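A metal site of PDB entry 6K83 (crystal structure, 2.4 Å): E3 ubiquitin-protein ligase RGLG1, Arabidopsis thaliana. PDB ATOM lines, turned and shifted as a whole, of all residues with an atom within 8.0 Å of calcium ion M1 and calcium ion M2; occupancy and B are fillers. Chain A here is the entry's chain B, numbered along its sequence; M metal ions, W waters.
The guanidinium group (NH2) of Arg 226 lies close to the backbone carbonyl oxygen (O) of Asp 220, 3.0 Å away. The backbone carbonyl oxygen (O) of Asp 229 sits at hydrogen-bond distance from the side-chain amide nitrogen (NE2) of Gln 264, at 2.8 Å. The side-chain amide nitrogen (NE2) of Gln 264 sits close to the backbone NH (N) of Phe 231. The side-chain amide oxygen (OE1) of Gln 264 lies close to the backbone carbonyl oxygen (O) of Glu 260, 3.4 Å away. N of Gln 232 is in hydrogen-bond range of O of Ile 203, at 2.9 Å. The side-chain carboxylate (OD2) of Asp 229 lies close to the backbone NH (N) of Ile 15, 2.8 Å away. The side-chain carboxylate of Asp 229 lies close to the guanidinium group of Arg 226. N of Phe 233 lies close to OD2 of Asp 220, at 3.4 Å.
Of the 25 residues printed, 4 come within 4 Å of calcium ion M1. The nearest printed residue that does not touch calcium ion M1 is Gln 232 (4.4 Å).
Of the 25 residues printed, 3 come within 4 Å of calcium ion M2.
Calcium ion M1 is bound by OE2 of Glu 260 (2.3 Å), OD1 of Asp 220 (2.4 Å), O of Phe 231 (2.4 Å), OD1 of Asp 229 (2.5 Å), O of Asp 220 (2.5 Å), OE1 of Glu 260 (2.6 Å), water W4 (2.6 Å) and OD2 of Asp 229 (2.6 Å).
Calcium ion M2 is bound by water W2, OE1 of Gln 232, OD2 of Asp 220, OD1 of Asp 220, water W1, OE2 of Glu 260 and water W3. Calcium ion M2 has seven donor atoms within binding distance. Slightly farther from calcium ion M2 lies water W4 (3.0 Å).
Water W4 lies within hydrogen-bond range of the side-chain carboxylate (OD1) of Asp 221 (2.5 Å), the backbone carbonyl oxygen (O) of Ile 15 (2.8 Å) and the side-chain amino group (NZ) of Lys 14 (3.3 Å).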
ATOM      1  N   SER A  13      20.684   9.164  -4.037  1.00  0.00           N
ATOM      2  CA  SER A  13      20.953  10.257  -3.115  1.00  0.00           C
ATOM      3  C   SER A  13      22.215  11.004  -3.535  1.00  0.00           C
ATOM      4  O   SER A  13      22.837  10.645  -4.535  1.00  0.00           O
ATOM      5  CB  SER A  13      21.096   9.725  -1.670  1.00  0.00           C
ATOM      6  OG  SER A  13      21.621  10.705  -0.785  1.00  0.00           O
ATOM      7  N   LYS A  14      22.587  12.035  -2.781  1.00  0.00           N
ATOM      8  CA  LYS A  14      23.823  12.776  -2.995  1.00  0.00           C
ATOM      9  C   LYS A  14      24.931  12.299  -2.044  1.00  0.00           C
ATOM     10  O   LYS A  14      24.723  12.214  -0.827  1.00  0.00           O
ATOM     11  CB  LYS A  14      23.579  14.262  -2.808  1.00  0.00           C
ATOM     12  CG  LYS A  14      24.857  15.072  -2.624  1.00  0.00           C
ATOM     13  CD  LYS A  14      24.528  16.516  -2.268  1.00  0.00           C
ATOM     14  CE  LYS A  14      25.588  17.095  -1.357  1.00  0.00           C
ATOM     15  NZ  LYS A  14      26.871  16.309  -1.461  1.00  0.00           N
ATOM     16  N   ILE A  15      26.101  12.017  -2.613  1.00  0.00           N
ATOM     17  CA  ILE A  15      27.263  11.476  -1.892  1.00  0.00           C
ATOM     18  C   ILE A  15      28.189  12.556  -1.306  1.00  0.00           C
ATOM     19  O   ILE A  15      28.836  13.329  -2.033  1.00  0.00           O
ATOM     20  CB  ILE A  15      28.108  10.579  -2.831  1.00  0.00           C
ATOM     21  CG1 ILE A  15      27.271   9.412  -3.365  1.00  0.00           C
ATOM     22  CG2 ILE A  15      29.364  10.072  -2.119  1.00  0.00           C
ATOM     23  CD1 ILE A  15      27.854   8.744  -4.615  1.00  0.00           C
ATOM     24  N   SER A  16      28.247  12.591   0.019  1.00  0.00           N
ATOM     25  CA  SER A  16      29.161  13.488   0.711  1.00  0.00           C
ATOM     26  C   SER A  16      30.583  12.926   0.694  1.00  0.00           C
ATOM     27  O   SER A  16      30.791  11.764   0.332  1.00  0.00           O
ATOM     28  CB  SER A  16      28.706  13.720   2.155  1.00  0.00           C
ATOM     29  OG  SER A  16      27.772  14.791   2.229  1.00  0.00           O
ATOM     30  N   ASP A  17      31.538  13.761   1.073  1.00  0.00           N
ATOM     31  CA  ASP A  17      32.902  13.304   1.301  1.00  0.00           C
ATOM     32  C   ASP A  17      32.941  12.430   2.550  1.00  0.00           C
ATOM     33  O   ASP A  17      32.770  12.919   3.666  1.00  0.00           O
ATOM     34  CB  ASP A  17      33.844  14.504   1.433  1.00  0.00           C
ATOM     35  CG  ASP A  17      33.824  15.396   0.217  1.00  0.00           C
ATOM     36  OD1 ASP A  17      32.942  15.191  -0.658  1.00  0.00           O
ATOM     37  OD2 ASP A  17      34.661  16.306   0.118  1.00  0.00           O
ATOM     38  N   ILE A 203      31.667   9.704 -13.270  1.00  0.00           N
ATOM     39  CA  ILE A 203      32.227  10.857 -13.958  1.00  0.00           C
ATOM     40  C   ILE A 203      33.054  11.662 -12.968  1.00  0.00           C
ATOM     41  O   ILE A 203      32.629  11.892 -11.846  1.00  0.00           O
ATOM     42  CB  ILE A 203      31.128  11.738 -14.604  1.00  0.00           C
ATOM     43  CG1 ILE A 203      30.220  10.872 -15.488  1.00  0.00           C
ATOM     44  CG2 ILE A 203      31.753  12.858 -15.436  1.00  0.00           C
ATOM     45  CD1 ILE A 203      28.967  11.557 -15.984  1.00  0.00           C
ATOM     46  N   MET A 216      29.796  23.434 -12.000  1.00  0.00           N
ATOM     47  CA  MET A 216      30.395  22.131 -11.776  1.00  0.00           C
ATOM     48  C   MET A 216      29.934  21.598 -10.440  1.00  0.00           C
ATOM     49  O   MET A 216      29.612  20.429 -10.337  1.00  0.00           O
ATOM     50  CB  MET A 216      31.911  22.224 -11.864  1.00  0.00           C
ATOM     51  CG  MET A 216      32.437  22.708 -13.228  1.00  0.00           C
ATOM     52  SD  MET A 216      31.948  21.658 -14.616  1.00  0.00           S
ATOM     53  CE  MET A 216      30.481  22.507 -15.217  1.00  0.00           C
ATOM     54  N   GLN A 217      29.860  22.465  -9.425  1.00  0.00           N
ATOM     55  CA  GLN A 217      29.353  22.063  -8.117  1.00  0.00           C
ATOM     56  C   GLN A 217      27.889  21.622  -8.200  1.00  0.00           C
ATOM     57  O   GLN A 217      27.483  20.747  -7.446  1.00  0.00           O
ATOM     58  CB  GLN A 217      29.524  23.180  -7.099  1.00  0.00           C
ATOM     59  CG  GLN A 217      30.945  23.369  -6.600  1.00  0.00           C
ATOM     60  CD  GLN A 217      31.265  24.824  -6.248  1.00  0.00           C
ATOM     61  OE1 GLN A 217      30.508  25.748  -6.561  1.00  0.00           O
ATOM     62  NE2 GLN A 217      32.407  25.034  -5.604  1.00  0.00           N
ATOM     63  N   GLU A 218      27.110  22.223  -9.107  1.00  0.00           N
ATOM     64  CA  GLU A 218      25.726  21.795  -9.324  1.00  0.00           C
ATOM     65  C   GLU A 218      25.688  20.378  -9.902  1.00  0.00           C
ATOM     66  O   GLU A 218      24.874  19.550  -9.483  1.00  0.00           O
ATOM     67  CB  GLU A 218      24.958  22.745 -10.258  1.00  0.00           C
ATOM     68  CG  GLU A 218      24.353  23.963  -9.576  1.00  0.00           C
ATOM     69  CD  GLU A 218      23.220  23.629  -8.601  1.00  0.00           C
ATOM     70  OE1 GLU A 218      22.310  22.863  -8.971  1.00  0.00           O
ATOM     71  OE2 GLU A 218      23.263  24.135  -7.463  1.00  0.00           O
ATOM     72  N   PHE A 219      26.560  20.119 -10.873  1.00  0.00           N
ATOM     73  CA  PHE A 219      26.648  18.794 -11.474  1.00  0.00           C
ATOM     74  C   PHE A 219      27.068  17.782 -10.400  1.00  0.00           C
ATOM     75  O   PHE A 219      26.563  16.656 -10.388  1.00  0.00           O
ATOM     76  CB  PHE A 219      27.607  18.773 -12.670  1.00  0.00           C
ATOM     77  CG  PHE A 219      27.102  19.571 -13.867  1.00  0.00           C
ATOM     78  CD1 PHE A 219      25.811  20.095 -13.884  1.00  0.00           C
ATOM     79  CD2 PHE A 219      27.909  19.799 -14.969  1.00  0.00           C
ATOM     80  CE1 PHE A 219      25.348  20.820 -14.965  1.00  0.00           C
ATOM     81  CE2 PHE A 219      27.442  20.527 -16.059  1.00  0.00           C
ATOM     82  CZ  PHE A 219      26.166  21.030 -16.055  1.00  0.00           C
ATOM     83  N   ASP A 220      27.952  18.196  -9.487  1.00  0.00           N
ATOM     84  CA  ASP A 220      28.463  17.309  -8.434  1.00  0.00           C
ATOM     85  C   ASP A 220      27.329  16.933  -7.462  1.00  0.00           C
ATOM     86  O   ASP A 220      27.081  15.758  -7.208  1.00  0.00           O
ATOM     87  CB  ASP A 220      29.620  17.996  -7.674  1.00  0.00           C
ATOM     88  CG  ASP A 220      30.332  17.072  -6.624  1.00  0.00           C
ATOM     89  OD1 ASP A 220      29.906  15.926  -6.412  1.00  0.00           O
ATOM     90  OD2 ASP A 220      31.328  17.508  -5.985  1.00  0.00           O
ATOM     91  N   ASP A 221      26.609  17.944  -6.980  1.00  0.00           N
ATOM     92  CA  ASP A 221      25.710  17.784  -5.845  1.00  0.00           C
ATOM     93  C   ASP A 221      24.215  17.798  -6.116  1.00  0.00           C
ATOM     94  O   ASP A 221      23.455  17.206  -5.343  1.00  0.00           O
ATOM     95  CB  ASP A 221      26.023  18.884  -4.825  1.00  0.00           C
ATOM     96  CG  ASP A 221      27.360  18.683  -4.156  1.00  0.00           C
ATOM     97  OD1 ASP A 221      27.695  17.519  -3.850  1.00  0.00           O
ATOM     98  OD2 ASP A 221      28.082  19.683  -3.951  1.00  0.00           O
ATOM     99  N   ASN A 222      23.772  18.478  -7.174  1.00  0.00           N
ATOM    100  CA  ASN A 222      22.328  18.700  -7.345  1.00  0.00           C
ATOM    101  C   ASN A 222      21.762  18.391  -8.728  1.00  0.00           C
ATOM    102  O   ASN A 222      21.463  19.317  -9.517  1.00  0.00           O
ATOM    103  CB  ASN A 222      21.991  20.147  -6.985  1.00  0.00           C
ATOM    104  CG  ASN A 222      20.489  20.426  -6.984  1.00  0.00           C
ATOM    105  OD1 ASN A 222      19.762  19.856  -6.171  1.00  0.00           O
ATOM    106  ND2 ASN A 222      20.027  21.275  -7.900  1.00  0.00           N
ATOM    107  N   ARG A 226      18.547  12.129 -11.774  1.00  0.00           N
ATOM    108  CA  ARG A 226      19.435  10.989 -12.046  1.00  0.00           C
ATOM    109  C   ARG A 226      19.278   9.893 -10.995  1.00  0.00           C
ATOM    110  O   ARG A 226      18.842  10.170  -9.876  1.00  0.00           O
ATOM    111  CB  ARG A 226      20.895  11.426 -12.129  1.00  0.00           C
ATOM    112  CG  ARG A 226      21.526  11.823 -10.804  1.00  0.00           C
ATOM    113  CD  ARG A 226      22.971  12.320 -10.984  1.00  0.00           C
ATOM    114  NE  ARG A 226      23.381  13.169  -9.872  1.00  0.00           N
ATOM    115  CZ  ARG A 226      24.484  13.927  -9.858  1.00  0.00           C
ATOM    116  NH1 ARG A 226      25.316  13.937 -10.900  1.00  0.00           N
ATOM    117  NH2 ARG A 226      24.749  14.674  -8.789  1.00  0.00           N
ATOM    118  N   PHE A 228      21.550   7.857  -9.622  1.00  0.00           N
ATOM    119  CA  PHE A 228      22.509   7.909  -8.527  1.00  0.00           C
ATOM    120  C   PHE A 228      23.488   9.021  -8.782  1.00  0.00           C
ATOM    121  O   PHE A 228      23.589   9.535  -9.903  1.00  0.00           O
ATOM    122  CB  PHE A 228      23.233   6.549  -8.343  1.00  0.00           C
ATOM    123  CG  PHE A 228      24.210   6.205  -9.435  1.00  0.00           C
ATOM    124  CD1 PHE A 228      23.821   5.453 -10.531  1.00  0.00           C
ATOM    125  CD2 PHE A 228      25.541   6.607  -9.354  1.00  0.00           C
ATOM    126  CE1 PHE A 228      24.745   5.109 -11.538  1.00  0.00           C
ATOM    127  CE2 PHE A 228      26.454   6.273 -10.343  1.00  0.00           C
ATOM    128  CZ  PHE A 228      26.061   5.525 -11.448  1.00  0.00           C
ATOM    129  N   ASP A 229      24.206   9.398  -7.737  1.00  0.00           N
ATOM    130  CA  ASP A 229      25.192  10.456  -7.813  1.00  0.00           C
ATOM    131  C   ASP A 229      26.425   9.958  -8.578  1.00  0.00           C
ATOM    132  O   ASP A 229      27.273   9.237  -8.013  1.00  0.00           O
ATOM    133  CB  ASP A 229      25.553  10.916  -6.397  1.00  0.00           C
ATOM    134  CG  ASP A 229      26.364  12.189  -6.384  1.00  0.00           C
ATOM    135  OD1 ASP A 229      26.757  12.658  -7.475  1.00  0.00           O
ATOM    136  OD2 ASP A 229      26.597  12.712  -5.281  1.00  0.00           O
ATOM    137  N   ASN A 230      26.497  10.323  -9.863  1.00  0.00           N
ATOM    138  CA  ASN A 230      27.547   9.786 -10.746  1.00  0.00           C
ATOM    139  C   ASN A 230      28.593  10.825 -11.115  1.00  0.00           C
ATOM    140  O   ASN A 230      29.424  10.566 -11.973  1.00  0.00           O
ATOM    141  CB  ASN A 230      26.938   9.232 -12.033  1.00  0.00           C
ATOM    142  CG  ASN A 230      26.113  10.269 -12.785  1.00  0.00           C
ATOM    143  OD1 ASN A 230      25.999  11.426 -12.356  1.00  0.00           O
ATOM    144  ND2 ASN A 230      25.512   9.858 -13.902  1.00  0.00           N
ATOM    145  N   PHE A 231      28.554  11.987 -10.488  1.00  0.00           N
ATOM    146  CA  PHE A 231      29.428  13.073 -10.894  1.00  0.00           C
ATOM    147  C   PHE A 231      30.194  13.617  -9.708  1.00  0.00           C
ATOM    148  O   PHE A 231      29.596  13.978  -8.704  1.00  0.00           O
ATOM    149  CB  PHE A 231      28.597  14.175 -11.543  1.00  0.00           C
ATOM    150  CG  PHE A 231      29.393  15.150 -12.383  1.00  0.00           C
ATOM    151  CD1 PHE A 231      30.146  16.148 -11.790  1.00  0.00           C
ATOM    152  CD2 PHE A 231      29.337  15.096 -13.771  1.00  0.00           C
ATOM    153  CE1 PHE A 231      30.829  17.055 -12.538  1.00  0.00           C
ATOM    154  CE2 PHE A 231      30.033  16.016 -14.552  1.00  0.00           C
ATOM    155  CZ  PHE A 231      30.782  16.999 -13.930  1.00  0.00           C
ATOM    156  N   GLN A 232      31.518  13.678  -9.832  1.00  0.00           N
ATOM    157  CA  GLN A 232      32.368  14.318  -8.818  1.00  0.00           C
ATOM    158  C   GLN A 232      33.160  15.507  -9.405  1.00  0.00           C
ATOM    159  O   GLN A 232      33.574  15.475 -10.566  1.00  0.00           O
ATOM    160  CB  GLN A 232      33.337  13.301  -8.186  1.00  0.00           C
ATOM    161  CG  GLN A 232      34.516  13.891  -7.367  1.00  0.00           C
ATOM    162  CD  GLN A 232      34.065  14.612  -6.077  1.00  0.00           C
ATOM    163  OE1 GLN A 232      32.971  15.143  -6.003  1.00  0.00           O
ATOM    164  NE2 GLN A 232      34.934  14.640  -5.071  1.00  0.00           N
ATOM    165  N   PHE A 233      33.345  16.560  -8.602  1.00  0.00           N
ATOM    166  CA  PHE A 233      34.065  17.752  -9.042  1.00  0.00           C
ATOM    167  C   PHE A 233      35.377  17.951  -8.281  1.00  0.00           C
ATOM    168  O   PHE A 233      35.406  17.954  -7.057  1.00  0.00           O
ATOM    169  CB  PHE A 233      33.191  19.011  -8.888  1.00  0.00           C
ATOM    170  CG  PHE A 233      33.964  20.306  -9.055  1.00  0.00           C
ATOM    171  CD1 PHE A 233      34.743  20.531 -10.194  1.00  0.00           C
ATOM    172  CD2 PHE A 233      33.899  21.291  -8.091  1.00  0.00           C
ATOM    173  CE1 PHE A 233      35.475  21.728 -10.346  1.00  0.00           C
ATOM    174  CE2 PHE A 233      34.619  22.482  -8.242  1.00  0.00           C
ATOM    175  CZ  PHE A 233      35.410  22.701  -9.376  1.00  0.00           C
ATOM    176  N   VAL A 234      36.454  18.134  -9.034  1.00  0.00           N
ATOM    177  CA  VAL A 234      37.749  18.365  -8.435  1.00  0.00           C
ATOM    178  C   VAL A 234      38.229  19.736  -8.864  1.00  0.00           C
ATOM    179  O   VAL A 234      38.336  19.993 -10.055  1.00  0.00           O
ATOM    180  CB  VAL A 234      38.770  17.270  -8.869  1.00  0.00           C
ATOM    181  CG1 VAL A 234      40.080  17.402  -8.097  1.00  0.00           C
ATOM    182  CG2 VAL A 234      38.152  15.894  -8.683  1.00  0.00           C
ATOM    183  N   SER A 256      40.519  13.390  -3.650  1.00  0.00           N
ATOM    184  CA  SER A 256      39.428  14.169  -4.191  1.00  0.00           C
ATOM    185  C   SER A 256      38.837  13.466  -5.424  1.00  0.00           C
ATOM    186  O   SER A 256      37.615  13.363  -5.560  1.00  0.00           O
ATOM    187  CB  SER A 256      39.895  15.575  -4.515  1.00  0.00           C
ATOM    188  OG  SER A 256      38.776  16.414  -4.659  1.00  0.00           O
ATOM    189  N   MET A 259      36.901  10.163  -4.265  1.00  0.00           N
ATOM    190  CA  MET A 259      36.035  10.325  -3.118  1.00  0.00           C
ATOM    191  C   MET A 259      34.664   9.672  -3.272  1.00  0.00           C
ATOM    192  O   MET A 259      34.077   9.187  -2.288  1.00  0.00           O
ATOM    193  CB  MET A 259      35.864  11.824  -2.818  1.00  0.00           C
ATOM    194  CG  MET A 259      35.038  12.138  -1.588  1.00  0.00           C
ATOM    195  SD  MET A 259      35.919  11.813  -0.053  1.00  0.00           S
ATOM    196  CE  MET A 259      37.129  13.139  -0.077  1.00  0.00           C
ATOM    197  N   GLU A 260      34.163   9.619  -4.499  1.00  0.00           N
ATOM    198  CA  GLU A 260      32.815   9.064  -4.738  1.00  0.00           C
ATOM    199  C   GLU A 260      32.853   7.702  -5.434  1.00  0.00           C
ATOM    200  O   GLU A 260      31.808   7.099  -5.692  1.00  0.00           O
ATOM    201  CB  GLU A 260      31.971  10.047  -5.557  1.00  0.00           C
ATOM    202  CG  GLU A 260      31.716  11.388  -4.862  1.00  0.00           C
ATOM    203  CD  GLU A 260      30.640  12.231  -5.563  1.00  0.00           C
ATOM    204  OE1 GLU A 260      29.863  11.695  -6.387  1.00  0.00           O
ATOM    205  OE2 GLU A 260      30.568  13.450  -5.283  1.00  0.00           O
ATOM    206  N   GLN A 264      29.713   4.943  -5.703  1.00  0.00           N
ATOM    207  CA  GLN A 264      29.196   4.885  -7.070  1.00  0.00           C
ATOM    208  C   GLN A 264      29.345   3.494  -7.670  1.00  0.00           C
ATOM    209  O   GLN A 264      28.511   3.050  -8.476  1.00  0.00           O
ATOM    210  CB  GLN A 264      29.908   5.897  -7.947  1.00  0.00           C
ATOM    211  CG  GLN A 264      29.503   7.329  -7.659  1.00  0.00           C
ATOM    212  CD  GLN A 264      30.379   8.305  -8.391  1.00  0.00           C
ATOM    213  OE1 GLN A 264      31.415   7.922  -8.928  1.00  0.00           O
ATOM    214  NE2 GLN A 264      29.980   9.579  -8.415  1.00  0.00           N
HETATM  215 CA    CA M   1      28.611  13.935  -6.478  1.00  0.00          CA
HETATM  216 CA    CA M   2      31.278  15.667  -4.497  1.00  0.00          CA
HETATM  217  O   HOH W   1      33.244  16.945  -4.104  1.00  0.00           O
HETATM  218  O   HOH W   2      30.292  17.315  -3.261  1.00  0.00           O
HETATM  219  O   HOH W   3      31.477  14.345  -2.102  1.00  0.00           O
HETATM  220  O   HOH W   4      28.312  15.111  -4.182  1.00  0.00           O
